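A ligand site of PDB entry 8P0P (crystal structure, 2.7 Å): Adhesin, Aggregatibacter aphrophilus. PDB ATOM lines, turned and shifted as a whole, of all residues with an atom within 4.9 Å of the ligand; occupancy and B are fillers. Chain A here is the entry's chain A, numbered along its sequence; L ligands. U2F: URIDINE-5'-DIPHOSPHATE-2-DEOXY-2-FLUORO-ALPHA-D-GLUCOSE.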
ATOM      1  N   MET A 219       7.556  -0.883 -12.542  1.00  0.00           N
ATOM      2  CA  MET A 219       6.367  -0.044 -12.638  1.00  0.00           C
ATOM      3  C   MET A 219       5.503  -0.518 -13.799  1.00  0.00           C
ATOM      4  O   MET A 219       4.286  -0.556 -13.674  1.00  0.00           O
ATOM      5  CB  MET A 219       6.730   1.434 -12.804  1.00  0.00           C
ATOM      6  CG  MET A 219       7.201   2.063 -11.528  1.00  0.00           C
ATOM      7  SD  MET A 219       7.480   3.847 -11.659  1.00  0.00           S
ATOM      8  CE  MET A 219       5.797   4.466 -11.750  1.00  0.00           C
ATOM      9  N   TYR A 223       0.605  -2.063 -16.436  1.00  0.00           N
ATOM     10  CA  TYR A 223      -0.109  -1.612 -17.613  1.00  0.00           C
ATOM     11  C   TYR A 223      -0.458  -2.779 -18.555  1.00  0.00           C
ATOM     12  O   TYR A 223      -1.157  -2.571 -19.544  1.00  0.00           O
ATOM     13  CB  TYR A 223       0.680  -0.490 -18.288  1.00  0.00           C
ATOM     14  CG  TYR A 223       1.008   0.694 -17.403  1.00  0.00           C
ATOM     15  CD1 TYR A 223       0.057   1.646 -17.097  1.00  0.00           C
ATOM     16  CD2 TYR A 223       2.281   0.907 -16.909  1.00  0.00           C
ATOM     17  CE1 TYR A 223       0.348   2.747 -16.294  1.00  0.00           C
ATOM     18  CE2 TYR A 223       2.603   2.006 -16.127  1.00  0.00           C
ATOM     19  CZ  TYR A 223       1.631   2.933 -15.803  1.00  0.00           C
ATOM     20  OH  TYR A 223       1.926   4.045 -15.019  1.00  0.00           O
ATOM     21  N   HIS A 277       4.354  18.161  -8.110  1.00  0.00           N
ATOM     22  CA  HIS A 277       4.091  16.761  -8.421  1.00  0.00           C
ATOM     23  C   HIS A 277       2.827  16.332  -7.673  1.00  0.00           C
ATOM     24  O   HIS A 277       2.461  16.968  -6.682  1.00  0.00           O
ATOM     25  CB  HIS A 277       5.341  15.910  -8.106  1.00  0.00           C
ATOM     26  CG  HIS A 277       5.326  14.568  -8.771  1.00  0.00           C
ATOM     27  ND1 HIS A 277       4.866  13.406  -8.172  1.00  0.00           N
ATOM     28  CD2 HIS A 277       5.675  14.230 -10.022  1.00  0.00           C
ATOM     29  CE1 HIS A 277       4.970  12.399  -9.025  1.00  0.00           C
ATOM     30  NE2 HIS A 277       5.452  12.877 -10.155  1.00  0.00           N
ATOM     31  N   SER A 278       2.150  15.268  -8.165  1.00  0.00           N
ATOM     32  CA  SER A 278       0.849  14.872  -7.624  1.00  0.00           C
ATOM     33  C   SER A 278       1.008  14.052  -6.350  1.00  0.00           C
ATOM     34  O   SER A 278       0.035  13.865  -5.628  1.00  0.00           O
ATOM     35  CB  SER A 278      -0.027  14.101  -8.604  1.00  0.00           C
ATOM     36  OG  SER A 278       0.694  13.050  -9.190  1.00  0.00           O
ATOM     37  N   ARG A 281       0.124  16.661  -3.902  1.00  0.00           N
ATOM     38  CA  ARG A 281      -1.268  17.048  -3.984  1.00  0.00           C
ATOM     39  C   ARG A 281      -2.179  15.999  -3.325  1.00  0.00           C
ATOM     40  O   ARG A 281      -3.278  16.358  -2.895  1.00  0.00           O
ATOM     41  CB  ARG A 281      -1.669  17.282  -5.444  1.00  0.00           C
ATOM     42  CG  ARG A 281      -1.132  18.564  -6.058  1.00  0.00           C
ATOM     43  CD  ARG A 281      -1.953  18.961  -7.279  1.00  0.00           C
ATOM     44  NE  ARG A 281      -1.918  17.944  -8.323  1.00  0.00           N
ATOM     45  CZ  ARG A 281      -0.940  17.803  -9.213  1.00  0.00           C
ATOM     46  NH1 ARG A 281       0.117  18.594  -9.186  1.00  0.00           N
ATOM     47  NH2 ARG A 281      -1.014  16.859 -10.142  1.00  0.00           N
ATOM     48  N   MET A 349       9.131   4.653  -8.627  1.00  0.00           N
ATOM     49  CA  MET A 349       9.625   5.709  -9.494  1.00  0.00           C
ATOM     50  C   MET A 349      11.133   5.824  -9.405  1.00  0.00           C
ATOM     51  O   MET A 349      11.774   6.161 -10.389  1.00  0.00           O
ATOM     52  CB  MET A 349       8.946   7.038  -9.153  1.00  0.00           C
ATOM     53  CG  MET A 349       7.499   7.043  -9.631  1.00  0.00           C
ATOM     54  SD  MET A 349       6.609   8.543  -9.209  1.00  0.00           S
ATOM     55  CE  MET A 349       4.990   7.886  -8.825  1.00  0.00           C
ATOM     56  N   GLY A 370       0.973   6.121  -4.671  1.00  0.00           N
ATOM     57  CA  GLY A 370       1.546   7.019  -5.664  1.00  0.00           C
ATOM     58  C   GLY A 370       1.755   6.311  -6.994  1.00  0.00           C
ATOM     59  O   GLY A 370       1.411   6.877  -8.024  1.00  0.00           O
ATOM     60  N   HIS A 371       2.314   5.091  -6.942  1.00  0.00           N
ATOM     61  CA  HIS A 371       2.165   4.112  -8.015  1.00  0.00           C
ATOM     62  C   HIS A 371       1.277   2.960  -7.523  1.00  0.00           C
ATOM     63  O   HIS A 371       1.713   2.142  -6.713  1.00  0.00           O
ATOM     64  CB  HIS A 371       3.501   3.571  -8.539  1.00  0.00           C
ATOM     65  CG  HIS A 371       3.386   2.582  -9.665  1.00  0.00           C
ATOM     66  ND1 HIS A 371       2.936   2.882 -10.932  1.00  0.00           N
ATOM     67  CD2 HIS A 371       3.698   1.280  -9.697  1.00  0.00           C
ATOM     68  CE1 HIS A 371       3.016   1.787 -11.706  1.00  0.00           C
ATOM     69  NE2 HIS A 371       3.453   0.797 -10.960  1.00  0.00           N
ATOM     70  N   PRO A 372       0.020   2.897  -8.017  1.00  0.00           N
ATOM     71  CA  PRO A 372      -1.010   2.019  -7.461  1.00  0.00           C
ATOM     72  C   PRO A 372      -0.938   0.543  -7.844  1.00  0.00           C
ATOM     73  O   PRO A 372      -1.830   0.021  -8.515  1.00  0.00           O
ATOM     74  CB  PRO A 372      -2.298   2.648  -7.997  1.00  0.00           C
ATOM     75  CG  PRO A 372      -1.872   3.123  -9.338  1.00  0.00           C
ATOM     76  CD  PRO A 372      -0.510   3.738  -9.093  1.00  0.00           C
ATOM     77  N   THR A 438      -1.629   9.221 -20.397  1.00  0.00           N
ATOM     78  CA  THR A 438      -0.202   9.096 -20.663  1.00  0.00           C
ATOM     79  C   THR A 438       0.016   7.867 -21.531  1.00  0.00           C
ATOM     80  O   THR A 438      -0.901   7.089 -21.672  1.00  0.00           O
ATOM     81  CB  THR A 438       0.602   9.066 -19.359  1.00  0.00           C
ATOM     82  OG1 THR A 438       0.004   8.099 -18.517  1.00  0.00           O
ATOM     83  CG2 THR A 438       0.622  10.415 -18.674  1.00  0.00           C
ATOM     84  N   LYS A 441      -0.686   4.059 -20.673  1.00  0.00           N
ATOM     85  CA  LYS A 441      -2.051   3.587 -20.524  1.00  0.00           C
ATOM     86  C   LYS A 441      -2.692   3.170 -21.845  1.00  0.00           C
ATOM     87  O   LYS A 441      -3.835   2.752 -21.837  1.00  0.00           O
ATOM     88  CB  LYS A 441      -2.919   4.669 -19.888  1.00  0.00           C
ATOM     89  CG  LYS A 441      -2.400   5.177 -18.550  1.00  0.00           C
ATOM     90  CD  LYS A 441      -3.252   6.283 -17.982  1.00  0.00           C
ATOM     91  CE  LYS A 441      -2.880   6.650 -16.558  1.00  0.00           C
ATOM     92  NZ  LYS A 441      -3.377   7.993 -16.230  1.00  0.00           N
ATOM     93  N   ALA A 466      -4.878  13.493 -25.651  1.00  0.00           N
ATOM     94  CA  ALA A 466      -3.901  14.330 -24.968  1.00  0.00           C
ATOM     95  C   ALA A 466      -2.859  13.437 -24.309  1.00  0.00           C
ATOM     96  O   ALA A 466      -3.091  12.889 -23.237  1.00  0.00           O
ATOM     97  CB  ALA A 466      -4.632  15.152 -23.949  1.00  0.00           C
ATOM     98  N   LEU A 467      -1.685  13.323 -24.929  1.00  0.00           N
ATOM     99  CA  LEU A 467      -0.805  12.182 -24.704  1.00  0.00           C
ATOM    100  C   LEU A 467       0.388  12.539 -23.803  1.00  0.00           C
ATOM    101  O   LEU A 467       1.483  12.838 -24.281  1.00  0.00           O
ATOM    102  CB  LEU A 467      -0.345  11.683 -26.083  1.00  0.00           C
ATOM    103  CG  LEU A 467      -1.446  11.037 -26.917  1.00  0.00           C
ATOM    104  CD1 LEU A 467      -1.165  11.141 -28.386  1.00  0.00           C
ATOM    105  CD2 LEU A 467      -1.625   9.577 -26.541  1.00  0.00           C
ATOM    106  N   GLY A 468       0.177  12.500 -22.498  1.00  0.00           N
ATOM    107  CA  GLY A 468       1.302  12.710 -21.585  1.00  0.00           C
ATOM    108  C   GLY A 468       2.424  11.718 -21.872  1.00  0.00           C
ATOM    109  O   GLY A 468       2.140  10.569 -22.147  1.00  0.00           O
ATOM    110  N   PRO A 494       0.613  15.901 -28.791  1.00  0.00           N
ATOM    111  CA  PRO A 494       1.787  15.650 -27.965  1.00  0.00           C
ATOM    112  C   PRO A 494       1.580  16.109 -26.540  1.00  0.00           C
ATOM    113  O   PRO A 494       0.619  16.832 -26.245  1.00  0.00           O
ATOM    114  CB  PRO A 494       2.880  16.498 -28.628  1.00  0.00           C
ATOM    115  CG  PRO A 494       2.420  16.644 -30.048  1.00  0.00           C
ATOM    116  CD  PRO A 494       0.931  16.804 -29.906  1.00  0.00           C
ATOM    117  N   HIS A 495       2.491  15.645 -25.674  1.00  0.00           N
ATOM    118  CA  HIS A 495       2.686  16.224 -24.356  1.00  0.00           C
ATOM    119  C   HIS A 495       2.730  17.738 -24.548  1.00  0.00           C
ATOM    120  O   HIS A 495       3.458  18.227 -25.381  1.00  0.00           O
ATOM    121  CB  HIS A 495       3.919  15.618 -23.693  1.00  0.00           C
ATOM    122  CG  HIS A 495       4.051  15.943 -22.247  1.00  0.00           C
ATOM    123  ND1 HIS A 495       4.575  17.146 -21.831  1.00  0.00           N
ATOM    124  CD2 HIS A 495       3.751  15.267 -21.141  1.00  0.00           C
ATOM    125  CE1 HIS A 495       4.578  17.181 -20.513  1.00  0.00           C
ATOM    126  NE2 HIS A 495       4.077  16.062 -20.089  1.00  0.00           N
ATOM    127  N   SER A 496       1.863  18.450 -23.813  1.00  0.00           N
ATOM    128  CA  SER A 496       1.720  19.895 -23.887  1.00  0.00           C
ATOM    129  C   SER A 496       1.788  20.490 -22.471  1.00  0.00           C
ATOM    130  O   SER A 496       1.588  19.790 -21.472  1.00  0.00           O
ATOM    131  CB  SER A 496       0.431  20.278 -24.600  1.00  0.00           C
ATOM    132  OG  SER A 496      -0.603  19.321 -24.378  1.00  0.00           O
ATOM    133  N   PRO A 497       2.069  21.804 -22.345  1.00  0.00           N
ATOM    134  CA  PRO A 497       1.917  22.478 -21.062  1.00  0.00           C
ATOM    135  C   PRO A 497       0.479  22.388 -20.554  1.00  0.00           C
ATOM    136  O   PRO A 497      -0.454  22.269 -21.329  1.00  0.00           O
ATOM    137  CB  PRO A 497       2.250  23.945 -21.371  1.00  0.00           C
ATOM    138  CG  PRO A 497       3.003  23.911 -22.693  1.00  0.00           C
ATOM    139  CD  PRO A 497       2.514  22.686 -23.427  1.00  0.00           C
ATOM    140  N   TYR A 498       0.297  22.502 -19.239  1.00  0.00           N
ATOM    141  CA  TYR A 498      -0.986  22.177 -18.627  1.00  0.00           C
ATOM    142  C   TYR A 498      -2.141  22.967 -19.266  1.00  0.00           C
ATOM    143  O   TYR A 498      -3.179  22.395 -19.597  1.00  0.00           O
ATOM    144  CB  TYR A 498      -0.922  22.416 -17.120  1.00  0.00           C
ATOM    145  CG  TYR A 498      -2.207  22.113 -16.404  1.00  0.00           C
ATOM    146  CD1 TYR A 498      -2.608  20.803 -16.182  1.00  0.00           C
ATOM    147  CD2 TYR A 498      -3.025  23.126 -15.941  1.00  0.00           C
ATOM    148  CE1 TYR A 498      -3.768  20.510 -15.499  1.00  0.00           C
ATOM    149  CE2 TYR A 498      -4.199  22.851 -15.255  1.00  0.00           C
ATOM    150  CZ  TYR A 498      -4.568  21.535 -15.025  1.00  0.00           C
ATOM    151  OH  TYR A 498      -5.716  21.250 -14.362  1.00  0.00           O
ATOM    152  N   TYR A 501      -3.034  21.531 -22.725  1.00  0.00           N
ATOM    153  CA  TYR A 501      -3.712  20.282 -22.455  1.00  0.00           C
ATOM    154  C   TYR A 501      -5.188  20.547 -22.127  1.00  0.00           C
ATOM    155  O   TYR A 501      -6.065  19.979 -22.756  1.00  0.00           O
ATOM    156  CB  TYR A 501      -2.968  19.575 -21.316  1.00  0.00           C
ATOM    157  CG  TYR A 501      -3.711  18.510 -20.563  1.00  0.00           C
ATOM    158  CD1 TYR A 501      -3.701  17.193 -20.992  1.00  0.00           C
ATOM    159  CD2 TYR A 501      -4.393  18.798 -19.409  1.00  0.00           C
ATOM    160  CE1 TYR A 501      -4.375  16.194 -20.314  1.00  0.00           C
ATOM    161  CE2 TYR A 501      -5.071  17.811 -18.719  1.00  0.00           C
ATOM    162  CZ  TYR A 501      -5.062  16.497 -19.167  1.00  0.00           C
ATOM    163  OH  TYR A 501      -5.728  15.493 -18.490  1.00  0.00           O
ATOM    164  N   PHE A 517      -5.352   0.288 -16.478  1.00  0.00           N
ATOM    165  CA  PHE A 517      -4.885   1.377 -15.642  1.00  0.00           C
ATOM    166  C   PHE A 517      -5.567   2.688 -16.031  1.00  0.00           C
ATOM    167  O   PHE A 517      -5.327   3.213 -17.127  1.00  0.00           O
ATOM    168  CB  PHE A 517      -3.376   1.527 -15.831  1.00  0.00           C
ATOM    169  CG  PHE A 517      -2.620   2.160 -14.715  1.00  0.00           C
ATOM    170  CD1 PHE A 517      -2.898   3.454 -14.311  1.00  0.00           C
ATOM    171  CD2 PHE A 517      -1.600   1.459 -14.079  1.00  0.00           C
ATOM    172  CE1 PHE A 517      -2.183   4.039 -13.271  1.00  0.00           C
ATOM    173  CE2 PHE A 517      -0.868   2.061 -13.068  1.00  0.00           C
ATOM    174  CZ  PHE A 517      -1.156   3.338 -12.666  1.00  0.00           C
ATOM    175  N   THR A 520      -6.821   9.491 -12.634  1.00  0.00           N
ATOM    176  CA  THR A 520      -7.079  10.081 -11.340  1.00  0.00           C
ATOM    177  C   THR A 520      -7.111  11.581 -11.571  1.00  0.00           C
ATOM    178  O   THR A 520      -8.181  12.164 -11.697  1.00  0.00           O
ATOM    179  CB  THR A 520      -6.033   9.673 -10.279  1.00  0.00           C
ATOM    180  OG1 THR A 520      -5.792   8.274 -10.333  1.00  0.00           O
ATOM    181  CG2 THR A 520      -6.463  10.019  -8.873  1.00  0.00           C
ATOM    182  N   ASN A 521      -5.927  12.169 -11.759  1.00  0.00           N
ATOM    183  CA  ASN A 521      -5.844  13.598 -12.044  1.00  0.00           C
ATOM    184  C   ASN A 521      -6.630  13.938 -13.305  1.00  0.00           C
ATOM    185  O   ASN A 521      -7.170  15.039 -13.374  1.00  0.00           O
ATOM    186  CB  ASN A 521      -4.418  14.095 -12.273  1.00  0.00           C
ATOM    187  CG  ASN A 521      -3.417  13.580 -11.256  1.00  0.00           C
ATOM    188  OD1 ASN A 521      -3.296  14.146 -10.170  1.00  0.00           O
ATOM    189  ND2 ASN A 521      -2.660  12.567 -11.656  1.00  0.00           N
ATOM    190  N   GLY A 522      -6.680  13.035 -14.300  1.00  0.00           N
ATOM    191  CA  GLY A 522      -7.458  13.243 -15.519  1.00  0.00           C
ATOM    192  C   GLY A 522      -8.957  13.449 -15.259  1.00  0.00           C
ATOM    193  O   GLY A 522      -9.636  14.145 -16.018  1.00  0.00           O
ATOM    194  N   ASP A 525      -9.273  16.884 -13.834  1.00  0.00           N
ATOM    195  CA  ASP A 525      -9.224  17.684 -15.046  1.00  0.00           C
ATOM    196  C   ASP A 525     -10.595  17.655 -15.724  1.00  0.00           C
ATOM    197  O   ASP A 525     -11.104  18.702 -16.115  1.00  0.00           O
ATOM    198  CB  ASP A 525      -8.094  17.215 -15.967  1.00  0.00           C
ATOM    199  CG  ASP A 525      -6.693  17.401 -15.400  1.00  0.00           C
ATOM    200  OD1 ASP A 525      -6.427  18.501 -14.849  1.00  0.00           O
ATOM    201  OD2 ASP A 525      -5.861  16.438 -15.512  1.00  0.00           O
HETATM  202  C1  U2F L   1       0.177  10.373 -11.987  1.00  0.00           C
HETATM  203  O1  U2F L   1       0.041  10.447 -13.377  1.00  0.00           O
HETATM  204  PB  U2F L   1      -1.299  10.032 -14.140  1.00  0.00           P
HETATM  205  O1B U2F L   1      -1.162   8.604 -14.538  1.00  0.00           O
HETATM  206  O2B U2F L   1      -2.493  10.517 -13.366  1.00  0.00           O
HETATM  207  O3A U2F L   1      -1.053  10.892 -15.441  1.00  0.00           O
HETATM  208  PA  U2F L   1      -1.910  12.200 -15.663  1.00  0.00           P
HETATM  209  O1A U2F L   1      -3.319  11.924 -15.212  1.00  0.00           O
HETATM  210  O2A U2F L   1      -1.588  12.782 -16.995  1.00  0.00           O
HETATM  211  O5' U2F L   1      -1.189  13.086 -14.550  1.00  0.00           O
HETATM  212  C5' U2F L   1      -0.098  13.931 -14.991  1.00  0.00           C
HETATM  213  C4' U2F L   1      -0.563  15.341 -15.232  1.00  0.00           C
HETATM  214  O4' U2F L   1      -0.081  15.762 -16.532  1.00  0.00           O
HETATM  215  C1' U2F L   1      -0.985  16.685 -17.069  1.00  0.00           C
HETATM  216  C2' U2F L   1      -2.351  16.136 -16.668  1.00  0.00           C
HETATM  217  C3' U2F L   1      -2.077  15.647 -15.261  1.00  0.00           C
HETATM  218  O3' U2F L   1      -2.417  16.847 -14.585  1.00  0.00           O
HETATM  219  O2' U2F L   1      -3.299  17.174 -16.521  1.00  0.00           O
HETATM  220  N1  U2F L   1      -0.751  16.732 -18.525  1.00  0.00           N
HETATM  221  C6' U2F L   1      -0.160  17.875 -19.049  1.00  0.00           C
HETATM  222  O6' U2F L   1       0.139  18.852 -18.365  1.00  0.00           O
HETATM  223  N3  U2F L   1       0.059  17.850 -20.414  1.00  0.00           N
HETATM  224  C7' U2F L   1      -0.244  16.808 -21.279  1.00  0.00           C
HETATM  225  O7' U2F L   1      -0.027  16.931 -22.481  1.00  0.00           O
HETATM  226  C8' U2F L   1      -0.828  15.658 -20.645  1.00  0.00           C
HETATM  227  C9' U2F L   1      -1.048  15.667 -19.323  1.00  0.00           C
HETATM  228  C2  U2F L   1       1.436  11.129 -11.658  1.00  0.00           C
HETATM  229  F1  U2F L   1       1.386  12.378 -12.318  1.00  0.00           F
HETATM  230  C3  U2F L   1       2.688  10.395 -12.105  1.00  0.00           C
HETATM  231  O3  U2F L   1       3.809  11.040 -11.524  1.00  0.00           O
HETATM  232  C4  U2F L   1       2.646   8.927 -11.664  1.00  0.00           C
HETATM  233  O4  U2F L   1       3.717   8.228 -12.313  1.00  0.00           O
HETATM  234  C5  U2F L   1       1.317   8.244 -12.031  1.00  0.00           C
HETATM  235  C6  U2F L   1       1.161   6.840 -11.477  1.00  0.00           C
HETATM  236  O6  U2F L   1       2.423   6.192 -11.225  1.00  0.00           O
HETATM  237  O5  U2F L   1       0.219   9.027 -11.501  1.00  0.00           O
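OG of Ser 278 sits close to F1 of the ligand, 3.3 Å away. Residues that only touch the ligand: Tyr 501 (2.9 Å), His 495 (3.4 Å), Tyr 498 (3.5 Å), Thr 438 (3.6 Å), Gly 522 (3.7 Å), Met 349 (3.7 Å), Gly 468 (3.8 Å), Pro 494 (3.8 Å) and Met 219 (3.8 Å). Within 4 Å of the ligand: Met 219, His 277, Ser 278, Met 349, Gly 370, His 371, Thr 438, Lys 441, Gly 468, Pro 494, His 495, Ser 496, Tyr 498, Tyr 501, Asn 521, Gly 522 and Asp 525. The nearest printed residue that does not touch the ligand is Pro 497 (4.2 Å).
OG of Ser 496 lies within hydrogen-bond range of O of Pro 494, at 3.3 Å. The side-chain carboxylate (OD2) of Asp 525 is in hydrogen-bond range of the side-chain hydroxyl (OH) of Tyr 501 (3.1 Å). The side-chain hydroxyl of Tyr 498 sits at hydrogen-bond distance from the side-chain carboxylate of Asp 525, at 2.9 Å. The backbone carbonyl oxygen (O) of Met 219 sits at hydrogen-bond distance from a ring nitrogen (NE2) of His 371 (3.1 Å). The backbone NH of His 495 lies within hydrogen-bond range of the backbone carbonyl oxygen of Leu 467, 3.3 Å away. SD of Met 219 is in hydrogen-bond range of N of Met 349, at 3.5 Å.
The side-chain amide nitrogen (ND2) of Asn 521 sits at hydrogen-bond distance from an oxygen (O2B) of the ligand (2.7 Å). An oxygen (O7') of the ligand is in hydrogen-bond range of the backbone NH (N) of Ser 496 (2.8 Å). The backbone carbonyl oxygen of Ser 496 is in hydrogen-bond range of a nitrogen (N3) of the ligand (2.7 Å). The side-chain hydroxyl (OG) of Ser 496 lies within hydrogen-bond range of an oxygen (O7') of the ligand, at 3.1 Å. A ring nitrogen (NE2) of His 277 sits at hydrogen-bond distance from an oxygen (O3) of the ligand, at 2.8 Å. The side-chain carboxylate (OD2) of Asp 525 is in hydrogen-bond range of an oxygen (O2') of the ligand (2.9 Å). The side-chain amino group (NZ) of Lys 441 is in salt-bridge range of an oxygen (O1B) of the ligand (2.9 Å). ND1 of His 371 is in hydrogen-bond range of O6 of the ligand (3.4 Å). O6 of the ligand sits at hydrogen-bond distance from O of Gly 370.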
